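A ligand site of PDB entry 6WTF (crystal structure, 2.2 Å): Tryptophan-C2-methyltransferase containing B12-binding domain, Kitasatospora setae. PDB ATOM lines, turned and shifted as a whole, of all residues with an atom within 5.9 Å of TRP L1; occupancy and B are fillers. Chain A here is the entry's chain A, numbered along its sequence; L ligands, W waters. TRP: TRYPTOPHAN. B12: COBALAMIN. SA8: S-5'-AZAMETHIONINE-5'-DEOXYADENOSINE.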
ATOM      1  N   THR A  73      14.339 -34.423 -30.857  1.00  0.00           N
ATOM      2  CA  THR A  73      15.269 -33.303 -30.967  1.00  0.00           C
ATOM      3  C   THR A  73      14.840 -32.084 -30.182  1.00  0.00           C
ATOM      4  O   THR A  73      15.663 -31.184 -29.963  1.00  0.00           O
ATOM      5  CB  THR A  73      15.463 -32.898 -32.437  1.00  0.00           C
ATOM      6  OG1 THR A  73      14.182 -32.658 -33.035  1.00  0.00           O
ATOM      7  CG2 THR A  73      16.189 -33.996 -33.200  1.00  0.00           C
ATOM      8  N   VAL A  74      13.577 -32.023 -29.737  1.00  0.00           N
ATOM      9  CA  VAL A  74      13.012 -30.880 -29.033  1.00  0.00           C
ATOM     10  C   VAL A  74      13.202 -29.621 -29.878  1.00  0.00           C
ATOM     11  O   VAL A  74      13.676 -28.586 -29.391  1.00  0.00           O
ATOM     12  CB  VAL A  74      13.611 -30.751 -27.617  1.00  0.00           C
ATOM     13  CG1 VAL A  74      12.831 -29.719 -26.780  1.00  0.00           C
ATOM     14  CG2 VAL A  74      13.581 -32.095 -26.930  1.00  0.00           C
ATOM     15  N   TYR A  75      12.838 -29.719 -31.145  1.00  0.00           N
ATOM     16  CA  TYR A  75      12.857 -28.584 -32.074  1.00  0.00           C
ATOM     17  C   TYR A  75      11.478 -28.513 -32.723  1.00  0.00           C
ATOM     18  O   TYR A  75      11.129 -29.375 -33.539  1.00  0.00           O
ATOM     19  CB  TYR A  75      13.966 -28.739 -33.114  1.00  0.00           C
ATOM     20  CG  TYR A  75      14.364 -27.439 -33.769  1.00  0.00           C
ATOM     21  CD1 TYR A  75      15.021 -26.449 -33.041  1.00  0.00           C
ATOM     22  CD2 TYR A  75      14.076 -27.186 -35.097  1.00  0.00           C
ATOM     23  CE1 TYR A  75      15.370 -25.242 -33.626  1.00  0.00           C
ATOM     24  CE2 TYR A  75      14.432 -25.996 -35.698  1.00  0.00           C
ATOM     25  CZ  TYR A  75      15.081 -25.025 -34.958  1.00  0.00           C
ATOM     26  OH  TYR A  75      15.433 -23.831 -35.546  1.00  0.00           O
ATOM     27  N   HIS A 268      32.505 -29.667 -21.444  1.00  0.00           N
ATOM     28  CA  HIS A 268      31.232 -28.974 -21.307  1.00  0.00           C
ATOM     29  C   HIS A 268      30.578 -29.409 -20.006  1.00  0.00           C
ATOM     30  O   HIS A 268      30.426 -30.612 -19.760  1.00  0.00           O
ATOM     31  CB  HIS A 268      30.305 -29.273 -22.485  1.00  0.00           C
ATOM     32  CG  HIS A 268      29.205 -28.270 -22.667  1.00  0.00           C
ATOM     33  ND1 HIS A 268      28.257 -28.024 -21.702  1.00  0.00           N
ATOM     34  CD2 HIS A 268      28.908 -27.456 -23.708  1.00  0.00           C
ATOM     35  CE1 HIS A 268      27.427 -27.091 -22.141  1.00  0.00           C
ATOM     36  NE2 HIS A 268      27.796 -26.737 -23.346  1.00  0.00           N
ATOM     37  N   TYR A 308      26.884 -23.762 -19.222  1.00  0.00           N
ATOM     38  CA  TYR A 308      25.546 -23.182 -19.309  1.00  0.00           C
ATOM     39  C   TYR A 308      25.353 -22.209 -18.154  1.00  0.00           C
ATOM     40  O   TYR A 308      25.778 -22.476 -17.032  1.00  0.00           O
ATOM     41  CB  TYR A 308      24.460 -24.255 -19.249  1.00  0.00           C
ATOM     42  CG  TYR A 308      24.085 -24.901 -20.562  1.00  0.00           C
ATOM     43  CD1 TYR A 308      23.970 -24.158 -21.724  1.00  0.00           C
ATOM     44  CD2 TYR A 308      23.843 -26.270 -20.634  1.00  0.00           C
ATOM     45  CE1 TYR A 308      23.622 -24.750 -22.934  1.00  0.00           C
ATOM     46  CE2 TYR A 308      23.496 -26.873 -21.824  1.00  0.00           C
ATOM     47  CZ  TYR A 308      23.393 -26.124 -22.968  1.00  0.00           C
ATOM     48  OH  TYR A 308      23.043 -26.736 -24.148  1.00  0.00           O
ATOM     49  N   ASN A 331      27.160 -20.145 -22.621  1.00  0.00           N
ATOM     50  CA  ASN A 331      25.836 -20.106 -23.238  1.00  0.00           C
ATOM     51  C   ASN A 331      24.857 -19.650 -22.165  1.00  0.00           C
ATOM     52  O   ASN A 331      24.723 -20.305 -21.134  1.00  0.00           O
ATOM     53  CB  ASN A 331      25.448 -21.467 -23.810  1.00  0.00           C
ATOM     54  CG  ASN A 331      24.076 -21.483 -24.450  1.00  0.00           C
ATOM     55  OD1 ASN A 331      23.078 -21.178 -23.801  1.00  0.00           O
ATOM     56  ND2 ASN A 331      24.019 -21.840 -25.720  1.00  0.00           N
ATOM     57  N   MET A 375      27.194 -17.204 -26.225  1.00  0.00           N
ATOM     58  CA  MET A 375      26.008 -17.475 -27.018  1.00  0.00           C
ATOM     59  C   MET A 375      24.792 -17.107 -26.194  1.00  0.00           C
ATOM     60  O   MET A 375      24.657 -17.535 -25.043  1.00  0.00           O
ATOM     61  CB  MET A 375      25.928 -18.938 -27.449  1.00  0.00           C
ATOM     62  CG  MET A 375      24.660 -19.206 -28.256  1.00  0.00           C
ATOM     63  SD  MET A 375      24.536 -20.886 -28.867  1.00  0.00           S
ATOM     64  CE  MET A 375      22.931 -20.838 -29.655  1.00  0.00           C
ATOM     65  N   GLU A 377      20.715 -17.233 -25.963  1.00  0.00           N
ATOM     66  CA  GLU A 377      19.552 -17.976 -26.434  1.00  0.00           C
ATOM     67  C   GLU A 377      18.305 -17.098 -26.423  1.00  0.00           C
ATOM     68  O   GLU A 377      18.094 -16.316 -25.494  1.00  0.00           O
ATOM     69  CB  GLU A 377      19.296 -19.215 -25.565  1.00  0.00           C
ATOM     70  CG  GLU A 377      20.463 -20.195 -25.444  1.00  0.00           C
ATOM     71  CD  GLU A 377      20.470 -21.246 -26.547  1.00  0.00           C
ATOM     72  OE1 GLU A 377      19.744 -21.082 -27.539  1.00  0.00           O
ATOM     73  OE2 GLU A 377      21.228 -22.235 -26.409  1.00  0.00           O
ATOM     74  N   SER A 408      15.320 -19.479 -31.598  1.00  0.00           N
ATOM     75  CA  SER A 408      14.431 -20.621 -31.790  1.00  0.00           C
ATOM     76  C   SER A 408      12.979 -20.154 -31.714  1.00  0.00           C
ATOM     77  O   SER A 408      12.660 -19.153 -31.075  1.00  0.00           O
ATOM     78  CB  SER A 408      14.710 -21.697 -30.730  1.00  0.00           C
ATOM     79  OG  SER A 408      16.092 -22.012 -30.702  1.00  0.00           O
ATOM     80  N   ASN A 527      19.244 -23.497 -34.734  1.00  0.00           N
ATOM     81  CA  ASN A 527      19.822 -23.796 -33.434  1.00  0.00           C
ATOM     82  C   ASN A 527      19.490 -25.243 -33.092  1.00  0.00           C
ATOM     83  O   ASN A 527      18.634 -25.499 -32.244  1.00  0.00           O
ATOM     84  CB  ASN A 527      19.269 -22.827 -32.371  1.00  0.00           C
ATOM     85  CG  ASN A 527      19.983 -22.935 -31.030  1.00  0.00           C
ATOM     86  OD1 ASN A 527      20.776 -23.841 -30.789  1.00  0.00           O
ATOM     87  ND2 ASN A 527      19.673 -21.997 -30.136  1.00  0.00           N
ATOM     88  N   ASN A 528      20.162 -26.187 -33.746  1.00  0.00           N
ATOM     89  CA  ASN A 528      19.847 -27.608 -33.629  1.00  0.00           C
ATOM     90  C   ASN A 528      21.118 -28.389 -33.934  1.00  0.00           C
ATOM     91  O   ASN A 528      21.599 -28.362 -35.064  1.00  0.00           O
ATOM     92  CB  ASN A 528      18.720 -28.007 -34.593  1.00  0.00           C
ATOM     93  CG  ASN A 528      18.199 -29.426 -34.355  1.00  0.00           C
ATOM     94  OD1 ASN A 528      18.816 -30.233 -33.674  1.00  0.00           O
ATOM     95  ND2 ASN A 528      17.025 -29.719 -34.921  1.00  0.00           N
ATOM     96  N   TYR A 529      21.662 -29.067 -32.928  1.00  0.00           N
ATOM     97  CA  TYR A 529      22.910 -29.792 -33.071  1.00  0.00           C
ATOM     98  C   TYR A 529      22.702 -31.260 -33.429  1.00  0.00           C
ATOM     99  O   TYR A 529      23.683 -31.984 -33.600  1.00  0.00           O
ATOM    100  CB  TYR A 529      23.740 -29.695 -31.789  1.00  0.00           C
ATOM    101  CG  TYR A 529      24.042 -28.281 -31.362  1.00  0.00           C
ATOM    102  CD1 TYR A 529      24.109 -27.248 -32.286  1.00  0.00           C
ATOM    103  CD2 TYR A 529      24.244 -27.962 -30.017  1.00  0.00           C
ATOM    104  CE1 TYR A 529      24.386 -25.941 -31.895  1.00  0.00           C
ATOM    105  CE2 TYR A 529      24.524 -26.669 -29.628  1.00  0.00           C
ATOM    106  CZ  TYR A 529      24.592 -25.662 -30.566  1.00  0.00           C
ATOM    107  OH  TYR A 529      24.862 -24.373 -30.164  1.00  0.00           O
ATOM    108  N   TRP A 548      28.766 -24.289 -30.967  1.00  0.00           N
ATOM    109  CA  TRP A 548      28.542 -22.926 -31.431  1.00  0.00           C
ATOM    110  C   TRP A 548      29.809 -22.090 -31.493  1.00  0.00           C
ATOM    111  O   TRP A 548      29.773 -20.973 -32.025  1.00  0.00           O
ATOM    112  CB  TRP A 548      27.513 -22.216 -30.536  1.00  0.00           C
ATOM    113  CG  TRP A 548      27.862 -22.160 -29.078  1.00  0.00           C
ATOM    114  CD1 TRP A 548      27.468 -23.048 -28.104  1.00  0.00           C
ATOM    115  CD2 TRP A 548      28.660 -21.172 -28.407  1.00  0.00           C
ATOM    116  NE1 TRP A 548      27.980 -22.668 -26.886  1.00  0.00           N
ATOM    117  CE2 TRP A 548      28.708 -21.517 -27.042  1.00  0.00           C
ATOM    118  CE3 TRP A 548      29.335 -20.028 -28.843  1.00  0.00           C
ATOM    119  CZ2 TRP A 548      29.412 -20.764 -26.112  1.00  0.00           C
ATOM    120  CZ3 TRP A 548      30.028 -19.279 -27.898  1.00  0.00           C
ATOM    121  CH2 TRP A 548      30.070 -19.658 -26.556  1.00  0.00           C
HETATM  122  N   TRP L   1      21.045 -24.270 -28.045  1.00  0.00           N
HETATM  123  CA  TRP L   1      21.671 -25.320 -27.245  1.00  0.00           C
HETATM  124  C   TRP L   1      23.152 -25.027 -27.056  1.00  0.00           C
HETATM  125  O   TRP L   1      23.807 -25.637 -26.206  1.00  0.00           O
HETATM  126  CB  TRP L   1      21.479 -26.698 -27.905  1.00  0.00           C
HETATM  127  CG  TRP L   1      20.056 -26.981 -28.314  1.00  0.00           C
HETATM  128  CD1 TRP L   1      19.545 -26.911 -29.566  1.00  0.00           C
HETATM  129  CD2 TRP L   1      18.970 -27.360 -27.446  1.00  0.00           C
HETATM  130  NE1 TRP L   1      18.206 -27.227 -29.551  1.00  0.00           N
HETATM  131  CE2 TRP L   1      17.832 -27.510 -28.262  1.00  0.00           C
HETATM  132  CE3 TRP L   1      18.857 -27.588 -26.078  1.00  0.00           C
HETATM  133  CZ2 TRP L   1      16.590 -27.873 -27.744  1.00  0.00           C
HETATM  134  CZ3 TRP L   1      17.622 -27.957 -25.563  1.00  0.00           C
HETATM  135  CH2 TRP L   1      16.507 -28.099 -26.397  1.00  0.00           C
HETATM  136  OXT TRP L   1      23.709 -24.180 -27.750  1.00  0.00           O
HETATM  137 CO   B12 L   2      21.251 -31.394 -24.451  1.00  0.00          CO
HETATM  138  N21 B12 L   2      19.546 -32.006 -23.924  1.00  0.00           N
HETATM  139  N22 B12 L   2      20.829 -31.846 -26.268  1.00  0.00           N
HETATM  140  N23 B12 L   2      23.121 -31.080 -24.759  1.00  0.00           N
HETATM  141  N24 B12 L   2      21.523 -31.209 -22.583  1.00  0.00           N
HETATM  142  C1  B12 L   2      19.251 -32.172 -22.511  1.00  0.00           C
HETATM  143  C20 B12 L   2      19.463 -33.635 -22.159  1.00  0.00           C
HETATM  144  C2  B12 L   2      17.767 -31.643 -22.396  1.00  0.00           C
HETATM  145  C25 B12 L   2      16.972 -32.215 -21.212  1.00  0.00           C
HETATM  146  C26 B12 L   2      17.686 -30.103 -22.337  1.00  0.00           C
HETATM  147  C27 B12 L   2      16.309 -29.567 -21.940  1.00  0.00           C
HETATM  148  O28 B12 L   2      15.342 -29.772 -22.681  1.00  0.00           O
HETATM  149  N29 B12 L   2      16.203 -28.903 -20.804  1.00  0.00           N
HETATM  150  C3  B12 L   2      17.189 -32.048 -23.796  1.00  0.00           C
HETATM  151  C30 B12 L   2      16.513 -33.432 -23.842  1.00  0.00           C
HETATM  152  C31 B12 L   2      14.980 -33.363 -23.857  1.00  0.00           C
HETATM  153  C32 B12 L   2      14.285 -34.693 -24.071  1.00  0.00           C
HETATM  154  O34 B12 L   2      14.918 -35.687 -24.421  1.00  0.00           O
HETATM  155  N33 B12 L   2      12.979 -34.711 -23.853  1.00  0.00           N
HETATM  156  C4  B12 L   2      18.451 -31.956 -24.626  1.00  0.00           C
HETATM  157  C5  B12 L   2      18.427 -31.830 -26.097  1.00  0.00           C
HETATM  158  C35 B12 L   2      17.041 -31.647 -26.636  1.00  0.00           C
HETATM  159  C6  B12 L   2      19.567 -31.903 -26.852  1.00  0.00           C
HETATM  160  C7  B12 L   2      19.718 -31.942 -28.368  1.00  0.00           C
HETATM  161  C36 B12 L   2      18.823 -32.998 -29.036  1.00  0.00           C
HETATM  162  C37 B12 L   2      19.484 -30.509 -28.916  1.00  0.00           C
HETATM  163  C38 B12 L   2      19.568 -30.447 -30.451  1.00  0.00           C
HETATM  164  O39 B12 L   2      20.667 -30.486 -31.020  1.00  0.00           O
HETATM  165  N40 B12 L   2      18.422 -30.348 -31.110  1.00  0.00           N
HETATM  166  C8  B12 L   2      21.218 -32.343 -28.537  1.00  0.00           C
HETATM  167  C41 B12 L   2      21.478 -33.857 -28.609  1.00  0.00           C
HETATM  168  C42 B12 L   2      22.953 -34.218 -28.777  1.00  0.00           C
HETATM  169  C43 B12 L   2      23.247 -35.709 -28.773  1.00  0.00           C
HETATM  170  O44 B12 L   2      22.549 -36.494 -28.121  1.00  0.00           O
HETATM  171  N45 B12 L   2      24.286 -36.097 -29.498  1.00  0.00           N
HETATM  172  C9  B12 L   2      21.763 -31.819 -27.229  1.00  0.00           C
HETATM  173  C10 B12 L   2      23.041 -31.310 -27.151  1.00  0.00           C
HETATM  174  C11 B12 L   2      23.637 -30.894 -25.978  1.00  0.00           C
HETATM  175  C12 B12 L   2      25.023 -30.276 -25.912  1.00  0.00           C
HETATM  176  C46 B12 L   2      25.977 -30.881 -26.951  1.00  0.00           C
HETATM  177  C47 B12 L   2      24.903 -28.766 -26.151  1.00  0.00           C
HETATM  178  C13 B12 L   2      25.483 -30.677 -24.478  1.00  0.00           C
HETATM  179  C48 B12 L   2      26.316 -31.958 -24.386  1.00  0.00           C
HETATM  180  C49 B12 L   2      27.759 -31.732 -23.927  1.00  0.00           C
HETATM  181  C50 B12 L   2      28.542 -33.002 -23.690  1.00  0.00           C
HETATM  182  O51 B12 L   2      28.077 -33.924 -23.024  1.00  0.00           O
HETATM  183  N52 B12 L   2      29.746 -33.048 -24.241  1.00  0.00           N
HETATM  184  C14 B12 L   2      24.112 -30.880 -23.793  1.00  0.00           C
HETATM  185  C15 B12 L   2      23.947 -30.837 -22.442  1.00  0.00           C
HETATM  186  C53 B12 L   2      25.133 -30.545 -21.563  1.00  0.00           C
HETATM  187  C16 B12 L   2      22.593 -31.141 -21.827  1.00  0.00           C
HETATM  188  C17 B12 L   2      22.294 -31.284 -20.336  1.00  0.00           C
HETATM  189  C54 B12 L   2      22.295 -29.910 -19.634  1.00  0.00           C
HETATM  190  C55 B12 L   2      23.194 -32.260 -19.523  1.00  0.00           C
HETATM  191  C56 B12 L   2      23.264 -33.669 -20.115  1.00  0.00           C
HETATM  192  C57 B12 L   2      24.172 -34.488 -19.234  1.00  0.00           C
HETATM  193  O58 B12 L   2      25.221 -34.972 -19.676  1.00  0.00           O
HETATM  194  N59 B12 L   2      23.790 -34.636 -17.970  1.00  0.00           N
HETATM  195  C18 B12 L   2      20.896 -31.931 -20.412  1.00  0.00           C
HETATM  196  C60 B12 L   2      19.953 -31.724 -19.209  1.00  0.00           C
HETATM  197  C61 B12 L   2      20.443 -32.323 -17.902  1.00  0.00           C
HETATM  198  O63 B12 L   2      20.841 -33.497 -17.866  1.00  0.00           O
HETATM  199  N62 B12 L   2      20.433 -31.527 -16.847  1.00  0.00           N
HETATM  200  C19 B12 L   2      20.337 -31.358 -21.720  1.00  0.00           C
HETATM  201  C1P B12 L   2      24.557 -35.388 -16.983  1.00  0.00           C
HETATM  202  C2P B12 L   2      24.307 -36.927 -17.134  1.00  0.00           C
HETATM  203  C3P B12 L   2      25.291 -37.704 -16.295  1.00  0.00           C
HETATM  204  O3  B12 L   2      23.034 -37.210 -16.607  1.00  0.00           O
HETATM  205  O4  B12 L   2      20.528 -37.456 -17.193  1.00  0.00           O
HETATM  206  O5  B12 L   2      22.286 -38.357 -18.742  1.00  0.00           O
HETATM  207  P   B12 L   2      21.885 -38.058 -17.306  1.00  0.00           P
HETATM  208  O2  B12 L   2      22.073 -39.465 -16.570  1.00  0.00           O
HETATM  209  C3R B12 L   2      21.637 -39.790 -15.265  1.00  0.00           C
HETATM  210  C2R B12 L   2      20.148 -40.120 -15.159  1.00  0.00           C
HETATM  211  O7R B12 L   2      19.462 -39.714 -16.339  1.00  0.00           O
HETATM  212  C1R B12 L   2      20.172 -41.645 -14.975  1.00  0.00           C
HETATM  213  O6R B12 L   2      21.366 -41.939 -14.280  1.00  0.00           O
HETATM  214  C4R B12 L   2      22.378 -41.041 -14.758  1.00  0.00           C
HETATM  215  C5R B12 L   2      23.394 -40.784 -13.668  1.00  0.00           C
HETATM  216  O8R B12 L   2      22.862 -39.975 -12.630  1.00  0.00           O
HETATM  217  N1B B12 L   2      20.127 -42.437 -16.202  1.00  0.00           N
HETATM  218  C8B B12 L   2      19.859 -43.796 -16.232  1.00  0.00           C
HETATM  219  C2B B12 L   2      20.606 -42.121 -17.448  1.00  0.00           C
HETATM  220  N3B B12 L   2      20.662 -43.138 -18.267  1.00  0.00           N
HETATM  221  C9B B12 L   2      20.199 -44.219 -17.513  1.00  0.00           C
HETATM  222  C4B B12 L   2      20.046 -45.555 -17.864  1.00  0.00           C
HETATM  223  C5B B12 L   2      19.546 -46.462 -16.930  1.00  0.00           C
HETATM  224  C5M B12 L   2      19.414 -47.911 -17.322  1.00  0.00           C
HETATM  225  C6B B12 L   2      19.198 -46.020 -15.634  1.00  0.00           C
HETATM  226  C6M B12 L   2      18.640 -46.988 -14.614  1.00  0.00           C
HETATM  227  C7B B12 L   2      19.364 -44.681 -15.287  1.00  0.00           C
HETATM  228  N   SA8 L   3      20.041 -26.620 -19.003  1.00  0.00           N
HETATM  229  CA  SA8 L   3      19.333 -25.928 -20.091  1.00  0.00           C
HETATM  230  C   SA8 L   3      19.113 -26.875 -21.266  1.00  0.00           C
HETATM  231  O   SA8 L   3      17.999 -26.638 -21.889  1.00  0.00           O
HETATM  232  OXT SA8 L   3      19.899 -27.749 -21.569  1.00  0.00           O
HETATM  233  CB  SA8 L   3      20.095 -24.653 -20.562  1.00  0.00           C
HETATM  234  CG  SA8 L   3      19.164 -23.598 -21.144  1.00  0.00           C
HETATM  235  ND  SA8 L   3      18.694 -23.911 -22.496  1.00  0.00           N
HETATM  236  CE  SA8 L   3      19.828 -24.023 -23.422  1.00  0.00           C
HETATM  237  C5' SA8 L   3      17.653 -22.986 -22.939  1.00  0.00           C
HETATM  238  C4' SA8 L   3      17.199 -23.234 -24.363  1.00  0.00           C
HETATM  239  O4' SA8 L   3      16.777 -24.614 -24.513  1.00  0.00           O
HETATM  240  C3' SA8 L   3      15.951 -22.442 -24.742  1.00  0.00           C
HETATM  241  O3' SA8 L   3      16.287 -21.110 -25.130  1.00  0.00           O
HETATM  242  C2' SA8 L   3      15.401 -23.259 -25.910  1.00  0.00           C
HETATM  243  O2' SA8 L   3      16.037 -22.899 -27.129  1.00  0.00           O
HETATM  244  C1' SA8 L   3      15.781 -24.694 -25.506  1.00  0.00           C
HETATM  245  N9  SA8 L   3      14.660 -25.481 -24.979  1.00  0.00           N
HETATM  246  C8  SA8 L   3      14.561 -26.042 -23.738  1.00  0.00           C
HETATM  247  N7  SA8 L   3      13.429 -26.675 -23.529  1.00  0.00           N
HETATM  248  C5  SA8 L   3      12.744 -26.535 -24.727  1.00  0.00           C
HETATM  249  C6  SA8 L   3      11.479 -26.982 -25.164  1.00  0.00           C
HETATM  250  N6  SA8 L   3      10.620 -27.662 -24.394  1.00  0.00           N
HETATM  251  N1  SA8 L   3      11.117 -26.687 -26.430  1.00  0.00           N
HETATM  252  C2  SA8 L   3      11.947 -25.976 -27.198  1.00  0.00           C
HETATM  253  N3  SA8 L   3      13.156 -25.482 -26.886  1.00  0.00           N
HETATM  254  C4  SA8 L   3      13.496 -25.800 -25.636  1.00  0.00           C
HETATM  255  O   HOH W   1      18.303 -24.148 -28.163  1.00  0.00           O
HETATM  256  O   HOH W   2      26.608 -25.767 -26.023  1.00  0.00           O
HETATM  257  O   HOH W   3      20.767 -28.767 -23.917  1.00  0.00           O
HETATM  258  O   HOH W   4      16.966 -24.628 -30.422  1.00  0.00           O
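Water W1 lies within hydrogen-bond range of a nitrogen (N) of TRP L1 (2.7 Å), an oxygen (O2') of SA8 L3 (2.8 Å), the side-chain amide nitrogen of Asn 527 (3.2 Å) and the side-chain carboxylate of Glu 377 (3.4 Å).
Water W2 lies within hydrogen-bond range of an oxygen (O) of TRP L1 (2.8 Å), a ring nitrogen (NE2) of His 268 (3.1 Å) and the indole nitrogen (NE1) of Trp 548 (3.5 Å).
Water W4 lies within hydrogen-bond range of O of Asn 527, OG of Ser 408 and NE1 of TRP L1.
Water W3 lies within hydrogen-bond range of OXT of SA8 L3 (2.7 Å) and OH of Tyr 308 (3.1 Å).
OH of Tyr 308 sits at hydrogen-bond distance from O of TRP L1 (2.5 Å).
The side-chain carboxylate of Glu 377 lies within salt-bridge range of a nitrogen (N) of TRP L1.
An oxygen (OXT) of TRP L1 sits at hydrogen-bond distance from the side-chain hydroxyl of Tyr 529, 2.7 Å away.
A nitrogen (NE1) of TRP L1 sits close to the backbone carbonyl oxygen (O) of Asn 527, at 3.2 Å.
OD1 of Asn 527 lies within hydrogen-bond range of N of TRP L1.
ND2 of Asn 331 sits at hydrogen-bond distance from OXT of TRP L1 (3.1 Å).
An oxygen (O39) of B12 L2 lies within hydrogen-bond range of the backbone NH (N) of Tyr 529 (2.6 Å).
A nitrogen (N40) of B12 L2 sits at hydrogen-bond distance from the backbone carbonyl oxygen of Thr 73 (3.1 Å).
A nitrogen (N40) of B12 L2 is in hydrogen-bond range of the side-chain amide oxygen of Asn 528, 2.6 Å away.
SD of Met 375 sits close to OXT of TRP L1.
Residues that only touch TRP L1: Val 74 (3.4 Å) and Trp 548 (3.9 Å).
Eight residues have an atom within 4 Å of TRP L1: Val 74, Tyr 308, Asn 331, Met 375, Glu 377, Asn 527, Tyr 529 and Trp 548.
A nitrogen (N29) of B12 L2 lies within hydrogen-bond range of an oxygen (O) of SA8 L3, 3.1 Å away.
The side-chain amide nitrogen of Asn 527 lies within hydrogen-bond range of the side-chain carboxylate of Glu 377, at 2.8 Å.
The side-chain amide nitrogen (ND2) of Asn 331 lies within hydrogen-bond range of the side-chain carboxylate (OE2) of Glu 377, 2.9 Å away.
The side-chain hydroxyl of Tyr 529 is in hydrogen-bond range of the side-chain sulfur of Met 375 (3.7 Å).
SD of Met 375 lies within hydrogen-bond range of ND2 of Asn 331 (3.3 Å).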
